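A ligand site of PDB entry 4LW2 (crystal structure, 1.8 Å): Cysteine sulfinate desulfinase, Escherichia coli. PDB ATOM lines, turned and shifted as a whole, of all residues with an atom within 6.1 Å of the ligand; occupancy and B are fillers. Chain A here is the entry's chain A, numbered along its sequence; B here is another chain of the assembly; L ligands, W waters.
N of Thr 94 is in hydrogen-bond range of O4 of the ligand, at 2.9 Å.
O3 of the ligand is in hydrogen-bond range of N of Thr 276 of chain B (2.9 Å).
OG1 of Thr 276 of chain B is in hydrogen-bond range of O3 of the ligand (2.5 Å).
The side-chain amide nitrogen (NE2) of Gln 202 sits at hydrogen-bond distance from an oxygen (O1) of the ligand (3.0 Å).
The side-chain hydroxyl (OG) of Ser 222 lies within hydrogen-bond range of an oxygen (O5) of the ligand, at 2.6 Å.
C5 of the ligand is bonded to NZ of Lys 225, at 1.4 Å.
The backbone NH (N) of Thr 93 lies within hydrogen-bond range of an oxygen (O4) of the ligand (3.4 Å).
A nitrogen (N1) of the ligand is in hydrogen-bond range of the side-chain carboxylate of Asp 199.
O4 of the ligand lies within hydrogen-bond range of OG1 of Thr 94, 2.6 Å away.
A ring nitrogen (NE2) of His 224 lies within hydrogen-bond range of the backbone carbonyl oxygen of Ala 30.
OG of Ser 222 sits at hydrogen-bond distance from OG1 of Thr 93 (2.7 Å).
The side-chain amide nitrogen (NE2) of Gln 202 lies within hydrogen-bond range of the backbone carbonyl oxygen (O) of Ala 29, 3.0 Å away.
A ring nitrogen (ND1) of His 122 sits at hydrogen-bond distance from the backbone NH (N) of Ala 124 (2.9 Å).
OD1 of Asp 199 is in hydrogen-bond range of N of Ala 201, 3.0 Å away.
Gly 92 touches the ligand.
His 122 touches the ligand (CB to N1, 3.4 Å).
Ala 124 touches the ligand (CB to C7, 3.7 Å).
Met 172 touches the ligand (O to C2, 3.9 Å).
CB of Asn 174 touches O1 of the ligand, at 3.4 Å.
CB of Ala 201 touches C3 of the ligand, at 3.3 Å.
His 224 touches the ligand.
Gly 275 of chain B touches the ligand (C to O3, 3.8 Å).
Hydrophobic or aromatic side chains within 4 Å of the ligand: His 122, Ala 124, Ala 201 and His 224.
Of the 25 residues printed, 15 come within 4 Å of the ligand.
The nearest printed residue that does not touch the ligand is Ala 29 (4.8 Å).
Water W2 lies within hydrogen-bond range of an oxygen (O4) of the ligand (2.8 Å) and the backbone carbonyl oxygen of Thr 276 of chain B (3.2 Å).
Water W1 lies within hydrogen-bond range of O5 of the ligand (2.9 Å), O of Arg 91 (3.0 Å) and ND1 of His 224 (3.4 Å).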
ATOM      1  N   ALA A  29       7.312 -21.595  39.316  1.00  0.00           N
ATOM      2  CA  ALA A  29       7.298 -22.361  38.029  1.00  0.00           C
ATOM      3  C   ALA A  29       5.874 -22.617  37.590  1.00  0.00           C
ATOM      4  O   ALA A  29       5.697 -23.011  36.444  1.00  0.00           O
ATOM      5  CB  ALA A  29       8.012 -23.730  38.205  1.00  0.00           C
ATOM      6  N   ALA A  30       4.912 -22.418  38.486  1.00  0.00           N
ATOM      7  CA  ALA A  30       3.474 -22.501  38.049  1.00  0.00           C
ATOM      8  C   ALA A  30       3.134 -21.119  37.535  1.00  0.00           C
ATOM      9  O   ALA A  30       2.625 -20.994  36.444  1.00  0.00           O
ATOM     10  CB  ALA A  30       2.510 -22.860  39.206  1.00  0.00           C
ATOM     11  N   ARG A  91      -2.146 -16.608  23.200  1.00  0.00           N
ATOM     12  CA  ARG A  91      -2.511 -16.462  24.601  1.00  0.00           C
ATOM     13  C   ARG A  91      -1.662 -17.308  25.524  1.00  0.00           C
ATOM     14  O   ARG A  91      -1.837 -17.287  26.693  1.00  0.00           O
ATOM     15  CB  ARG A  91      -3.987 -16.809  24.803  1.00  0.00           C
ATOM     16  CG  ARG A  91      -4.321 -18.267  24.502  1.00  0.00           C
ATOM     17  CD  ARG A  91      -5.803 -18.591  24.656  1.00  0.00           C
ATOM     18  NE  ARG A  91      -6.074 -20.004  24.385  1.00  0.00           N
ATOM     19  CZ  ARG A  91      -6.016 -20.958  25.300  1.00  0.00           C
ATOM     20  NH1 ARG A  91      -5.691 -20.670  26.553  1.00  0.00           N
ATOM     21  NH2 ARG A  91      -6.277 -22.223  24.969  1.00  0.00           N
ATOM     22  N   GLY A  92      -0.641 -17.842  25.041  1.00  0.00           N
ATOM     23  CA  GLY A  92       0.187 -18.655  25.865  1.00  0.00           C
ATOM     24  C   GLY A  92       0.939 -19.726  25.104  1.00  0.00           C
ATOM     25  O   GLY A  92       0.677 -19.949  23.974  1.00  0.00           O
ATOM     26  N   THR A  93       1.890 -20.365  25.783  1.00  0.00           N
ATOM     27  CA  THR A  93       2.693 -21.402  25.121  1.00  0.00           C
ATOM     28  C   THR A  93       1.763 -22.433  24.443  1.00  0.00           C
ATOM     29  O   THR A  93       2.026 -22.926  23.367  1.00  0.00           O
ATOM     30  CB  THR A  93       3.492 -22.172  26.189  1.00  0.00           C
ATOM     31  OG1 THR A  93       4.349 -21.211  26.860  1.00  0.00           O
ATOM     32  CG2 THR A  93       4.401 -23.278  25.548  1.00  0.00           C
ATOM     33  N   THR A  94       0.686 -22.819  25.167  1.00  0.00           N
ATOM     34  CA  THR A  94      -0.266 -23.763  24.565  1.00  0.00           C
ATOM     35  C   THR A  94      -0.773 -23.369  23.212  1.00  0.00           C
ATOM     36  O   THR A  94      -0.748 -24.154  22.273  1.00  0.00           O
ATOM     37  CB  THR A  94      -1.456 -24.056  25.566  1.00  0.00           C
ATOM     38  OG1 THR A  94      -0.908 -24.487  26.794  1.00  0.00           O
ATOM     39  CG2 THR A  94      -2.395 -25.200  25.014  1.00  0.00           C
ATOM     40  N   GLU A  95      -1.305 -22.157  23.074  1.00  0.00           N
ATOM     41  CA  GLU A  95      -1.764 -21.733  21.756  1.00  0.00           C
ATOM     42  C   GLU A  95      -0.631 -21.716  20.722  1.00  0.00           C
ATOM     43  O   GLU A  95      -0.806 -22.163  19.613  1.00  0.00           O
ATOM     44  CB  GLU A  95      -2.428 -20.373  21.818  1.00  0.00           C
ATOM     45  CG  GLU A  95      -2.983 -20.017  20.441  1.00  0.00           C
ATOM     46  CD  GLU A  95      -3.691 -18.640  20.395  1.00  0.00           C
ATOM     47  OE1 GLU A  95      -3.378 -17.657  21.131  1.00  0.00           O
ATOM     48  OE2 GLU A  95      -4.574 -18.546  19.532  1.00  0.00           O
ATOM     49  N   ILE A  97       1.949 -23.585  20.404  1.00  0.00           N
ATOM     50  CA  ILE A  97       2.310 -24.894  19.891  1.00  0.00           C
ATOM     51  C   ILE A  97       1.169 -25.437  19.013  1.00  0.00           C
ATOM     52  O   ILE A  97       1.418 -26.052  17.973  1.00  0.00           O
ATOM     53  CB  ILE A  97       2.693 -25.895  21.080  1.00  0.00           C
ATOM     54  CG1 ILE A  97       3.937 -25.351  21.857  1.00  0.00           C
ATOM     55  CG2 ILE A  97       2.817 -27.325  20.554  1.00  0.00           C
ATOM     56  CD1 ILE A  97       4.293 -26.209  23.178  1.00  0.00           C
ATOM     57  N   HIS A 122       5.690 -31.358  28.516  1.00  0.00           N
ATOM     58  CA  HIS A 122       4.404 -30.924  29.096  1.00  0.00           C
ATOM     59  C   HIS A 122       3.318 -31.284  28.116  1.00  0.00           C
ATOM     60  O   HIS A 122       3.570 -31.354  26.884  1.00  0.00           O
ATOM     61  CB  HIS A 122       4.539 -29.379  29.317  1.00  0.00           C
ATOM     62  CG  HIS A 122       3.386 -28.694  29.982  1.00  0.00           C
ATOM     63  ND1 HIS A 122       2.163 -28.486  29.357  1.00  0.00           N
ATOM     64  CD2 HIS A 122       3.333 -27.984  31.166  1.00  0.00           C
ATOM     65  CE1 HIS A 122       1.375 -27.774  30.163  1.00  0.00           C
ATOM     66  NE2 HIS A 122       2.056 -27.436  31.256  1.00  0.00           N
ATOM     67  N   ALA A 124       1.178 -29.578  26.801  1.00  0.00           N
ATOM     68  CA  ALA A 124       1.077 -28.583  25.742  1.00  0.00           C
ATOM     69  C   ALA A 124       1.864 -28.937  24.491  1.00  0.00           C
ATOM     70  O   ALA A 124       1.528 -28.520  23.439  1.00  0.00           O
ATOM     71  CB  ALA A 124       1.523 -27.201  26.239  1.00  0.00           C
ATOM     72  N   ASN A 125       2.960 -29.641  24.691  1.00  0.00           N
ATOM     73  CA  ASN A 125       3.844 -30.073  23.612  1.00  0.00           C
ATOM     74  C   ASN A 125       3.730 -31.592  23.308  1.00  0.00           C
ATOM     75  O   ASN A 125       4.603 -32.174  22.824  1.00  0.00           O
ATOM     76  CB  ASN A 125       5.278 -29.619  23.859  1.00  0.00           C
ATOM     77  CG  ASN A 125       6.131 -29.429  22.561  1.00  0.00           C
ATOM     78  OD1 ASN A 125       7.333 -29.467  22.620  1.00  0.00           O
ATOM     79  ND2 ASN A 125       5.502 -29.174  21.460  1.00  0.00           N
ATOM     80  N   MET A 172      13.350 -27.017  28.688  1.00  0.00           N
ATOM     81  CA  MET A 172      13.495 -27.201  30.132  1.00  0.00           C
ATOM     82  C   MET A 172      12.204 -27.771  30.690  1.00  0.00           C
ATOM     83  O   MET A 172      11.140 -27.192  30.437  1.00  0.00           O
ATOM     84  CB  MET A 172      13.757 -25.846  30.768  1.00  0.00           C
ATOM     85  CG  MET A 172      13.970 -25.961  32.288  1.00  0.00           C
ATOM     86  SD  MET A 172      14.433 -24.317  32.922  1.00  0.00           S
ATOM     87  CE  MET A 172      14.213 -24.581  34.626  1.00  0.00           C
ATOM     88  N   SER A 173      12.286 -28.885  31.434  1.00  0.00           N
ATOM     89  CA  SER A 173      11.082 -29.509  32.016  1.00  0.00           C
ATOM     90  C   SER A 173      10.556 -28.696  33.202  1.00  0.00           C
ATOM     91  O   SER A 173      11.338 -28.185  33.943  1.00  0.00           O
ATOM     92  CB  SER A 173      11.424 -30.924  32.506  1.00  0.00           C
ATOM     93  OG  SER A 173      10.421 -31.394  33.383  1.00  0.00           O
ATOM     94  N   ASN A 174       9.251 -28.567  33.337  1.00  0.00           N
ATOM     95  CA  ASN A 174       8.639 -27.931  34.527  1.00  0.00           C
ATOM     96  C   ASN A 174       8.593 -28.875  35.685  1.00  0.00           C
ATOM     97  O   ASN A 174       8.064 -28.503  36.725  1.00  0.00           O
ATOM     98  CB  ASN A 174       7.206 -27.433  34.199  1.00  0.00           C
ATOM     99  CG  ASN A 174       6.288 -28.589  33.879  1.00  0.00           C
ATOM    100  OD1 ASN A 174       6.680 -29.498  33.059  1.00  0.00           O
ATOM    101  ND2 ASN A 174       5.057 -28.481  34.374  1.00  0.00           N
ATOM    102  N   ASP A 199       9.622 -26.082  23.229  1.00  0.00           N
ATOM    103  CA  ASP A 199       8.734 -25.558  24.260  1.00  0.00           C
ATOM    104  C   ASP A 199       9.636 -24.853  25.271  1.00  0.00           C
ATOM    105  O   ASP A 199      10.408 -25.502  25.974  1.00  0.00           O
ATOM    106  CB  ASP A 199       7.971 -26.683  24.937  1.00  0.00           C
ATOM    107  CG  ASP A 199       7.173 -26.220  26.126  1.00  0.00           C
ATOM    108  OD1 ASP A 199       7.261 -25.045  26.502  1.00  0.00           O
ATOM    109  OD2 ASP A 199       6.406 -27.048  26.670  1.00  0.00           O
ATOM    110  N   GLY A 200       9.579 -23.511  25.228  1.00  0.00           N
ATOM    111  CA  GLY A 200      10.378 -22.621  26.104  1.00  0.00           C
ATOM    112  C   GLY A 200       9.660 -22.025  27.264  1.00  0.00           C
ATOM    113  O   GLY A 200      10.150 -21.007  27.840  1.00  0.00           O
ATOM    114  N   ALA A 201       8.512 -22.601  27.637  1.00  0.00           N
ATOM    115  CA  ALA A 201       7.737 -21.931  28.735  1.00  0.00           C
ATOM    116  C   ALA A 201       8.587 -21.774  30.004  1.00  0.00           C
ATOM    117  O   ALA A 201       8.445 -20.776  30.714  1.00  0.00           O
ATOM    118  CB  ALA A 201       6.421 -22.745  29.043  1.00  0.00           C
ATOM    119  N   GLN A 202       9.373 -22.803  30.401  1.00  0.00           N
ATOM    120  CA  GLN A 202      10.311 -22.630  31.501  1.00  0.00           C
ATOM    121  C   GLN A 202      11.642 -22.054  31.043  1.00  0.00           C
ATOM    122  O   GLN A 202      12.264 -21.197  31.699  1.00  0.00           O
ATOM    123  CB  GLN A 202      10.582 -23.947  32.257  1.00  0.00           C
ATOM    124  CG  GLN A 202       9.377 -24.597  32.893  1.00  0.00           C
ATOM    125  CD  GLN A 202       8.893 -23.783  34.043  1.00  0.00           C
ATOM    126  OE1 GLN A 202       9.686 -23.158  34.700  1.00  0.00           O
ATOM    127  NE2 GLN A 202       7.591 -23.840  34.303  1.00  0.00           N
ATOM    128  N   SER A 222       5.202 -18.388  27.749  1.00  0.00           N
ATOM    129  CA  SER A 222       4.035 -17.669  28.286  1.00  0.00           C
ATOM    130  C   SER A 222       4.476 -16.489  29.133  1.00  0.00           C
ATOM    131  O   SER A 222       5.431 -16.552  29.913  1.00  0.00           O
ATOM    132  CB  SER A 222       3.237 -18.622  29.206  1.00  0.00           C
ATOM    133  OG  SER A 222       2.692 -19.676  28.407  1.00  0.00           O
ATOM    134  N   HIS A 224       2.950 -15.267  31.789  1.00  0.00           N
ATOM    135  CA  HIS A 224       2.616 -15.225  33.229  1.00  0.00           C
ATOM    136  C   HIS A 224       3.746 -15.854  34.094  1.00  0.00           C
ATOM    137  O   HIS A 224       3.915 -15.531  35.268  1.00  0.00           O
ATOM    138  CB  HIS A 224       1.235 -15.902  33.456  1.00  0.00           C
ATOM    139  CG  HIS A 224       1.237 -17.393  33.303  1.00  0.00           C
ATOM    140  ND1 HIS A 224       0.956 -18.038  32.095  1.00  0.00           N
ATOM    141  CD2 HIS A 224       1.448 -18.384  34.214  1.00  0.00           C
ATOM    142  CE1 HIS A 224       1.006 -19.366  32.294  1.00  0.00           C
ATOM    143  NE2 HIS A 224       1.281 -19.594  33.563  1.00  0.00           N
ATOM    144  N   LYS A 225       4.519 -16.737  33.456  1.00  0.00           N
ATOM    145  CA  LYS A 225       5.698 -17.313  34.108  1.00  0.00           C
ATOM    146  C   LYS A 225       6.903 -16.362  34.021  1.00  0.00           C
ATOM    147  O   LYS A 225       7.827 -16.455  34.849  1.00  0.00           O
ATOM    148  CB  LYS A 225       6.008 -18.712  33.509  1.00  0.00           C
ATOM    149  CG  LYS A 225       4.932 -19.793  33.869  1.00  0.00           C
ATOM    150  CD  LYS A 225       5.107 -21.079  33.070  1.00  0.00           C
ATOM    151  CE  LYS A 225       4.023 -22.038  33.594  1.00  0.00           C
ATOM    152  NZ  LYS A 225       4.218 -23.269  32.752  1.00  0.00           N
ATOM    153  N   ALA B 274      -7.996 -25.300  26.788  1.00  0.00           N
ATOM    154  CA  ALA B 274      -6.615 -25.742  27.068  1.00  0.00           C
ATOM    155  C   ALA B 274      -5.705 -24.691  27.715  1.00  0.00           C
ATOM    156  O   ALA B 274      -5.809 -23.437  27.456  1.00  0.00           O
ATOM    157  CB  ALA B 274      -5.956 -26.122  25.708  1.00  0.00           C
ATOM    158  N   GLY B 275      -4.832 -25.206  28.553  1.00  0.00           N
ATOM    159  CA  GLY B 275      -3.675 -24.432  29.121  1.00  0.00           C
ATOM    160  C   GLY B 275      -4.152 -23.430  30.200  1.00  0.00           C
ATOM    161  O   GLY B 275      -5.273 -23.464  30.662  1.00  0.00           O
ATOM    162  N   THR B 276      -3.242 -22.592  30.620  1.00  0.00           N
ATOM    163  CA  THR B 276      -3.508 -21.682  31.755  1.00  0.00           C
ATOM    164  C   THR B 276      -4.531 -20.644  31.275  1.00  0.00           C
ATOM    165  O   THR B 276      -4.314 -20.019  30.202  1.00  0.00           O
ATOM    166  CB  THR B 276      -2.189 -20.942  32.162  1.00  0.00           C
ATOM    167  OG1 THR B 276      -1.199 -21.931  32.558  1.00  0.00           O
ATOM    168  CG2 THR B 276      -2.446 -19.986  33.406  1.00  0.00           C
ATOM    169  N   PRO B 277      -5.631 -20.486  32.036  1.00  0.00           N
ATOM    170  CA  PRO B 277      -6.618 -19.511  31.555  1.00  0.00           C
ATOM    171  C   PRO B 277      -6.029 -18.113  31.637  1.00  0.00           C
ATOM    172  O   PRO B 277      -5.072 -17.864  32.380  1.00  0.00           O
ATOM    173  CB  PRO B 277      -7.726 -19.564  32.635  1.00  0.00           C
ATOM    174  CG  PRO B 277      -7.540 -20.881  33.404  1.00  0.00           C
ATOM    175  CD  PRO B 277      -5.995 -21.106  33.324  1.00  0.00           C
HETATM  176  N1  LIG L   1       5.298 -26.098  28.823  1.00  0.00           N
HETATM  177  C1  LIG L   1       5.989 -25.981  29.945  1.00  0.00           C
HETATM  178  C2  LIG L   1       7.300 -26.603  30.076  1.00  0.00           C
HETATM  179  C3  LIG L   1       5.392 -25.171  30.950  1.00  0.00           C
HETATM  180  O1  LIG L   1       5.993 -25.033  32.095  1.00  0.00           O
HETATM  181  C4  LIG L   1       4.093 -24.598  30.739  1.00  0.00           C
HETATM  182  C5  LIG L   1       3.566 -23.768  31.629  1.00  0.00           C
HETATM  183  C6  LIG L   1       3.399 -24.778  29.523  1.00  0.00           C
HETATM  184  C7  LIG L   1       3.985 -25.562  28.524  1.00  0.00           C
HETATM  185  C8  LIG L   1       2.091 -24.305  29.200  1.00  0.00           C
HETATM  186  O2  LIG L   1       1.900 -22.855  29.396  1.00  0.00           O
HETATM  187  P1  LIG L   1       0.400 -22.160  29.322  1.00  0.00           P
HETATM  188  O3  LIG L   1      -0.407 -22.878  30.340  1.00  0.00           O
HETATM  189  O4  LIG L   1      -0.088 -22.275  27.857  1.00  0.00           O
HETATM  190  O5  LIG L   1       0.775 -20.770  29.781  1.00  0.00           O
HETATM  191  O   HOH W   1      -0.849 -18.423  29.276  1.00  0.00           O
HETATM  192  O   HOH W   2      -2.367 -20.711  27.709  1.00  0.00           O
HETATM  193  O   HOH W   3       1.336 -25.818  33.346  1.00  0.00           O
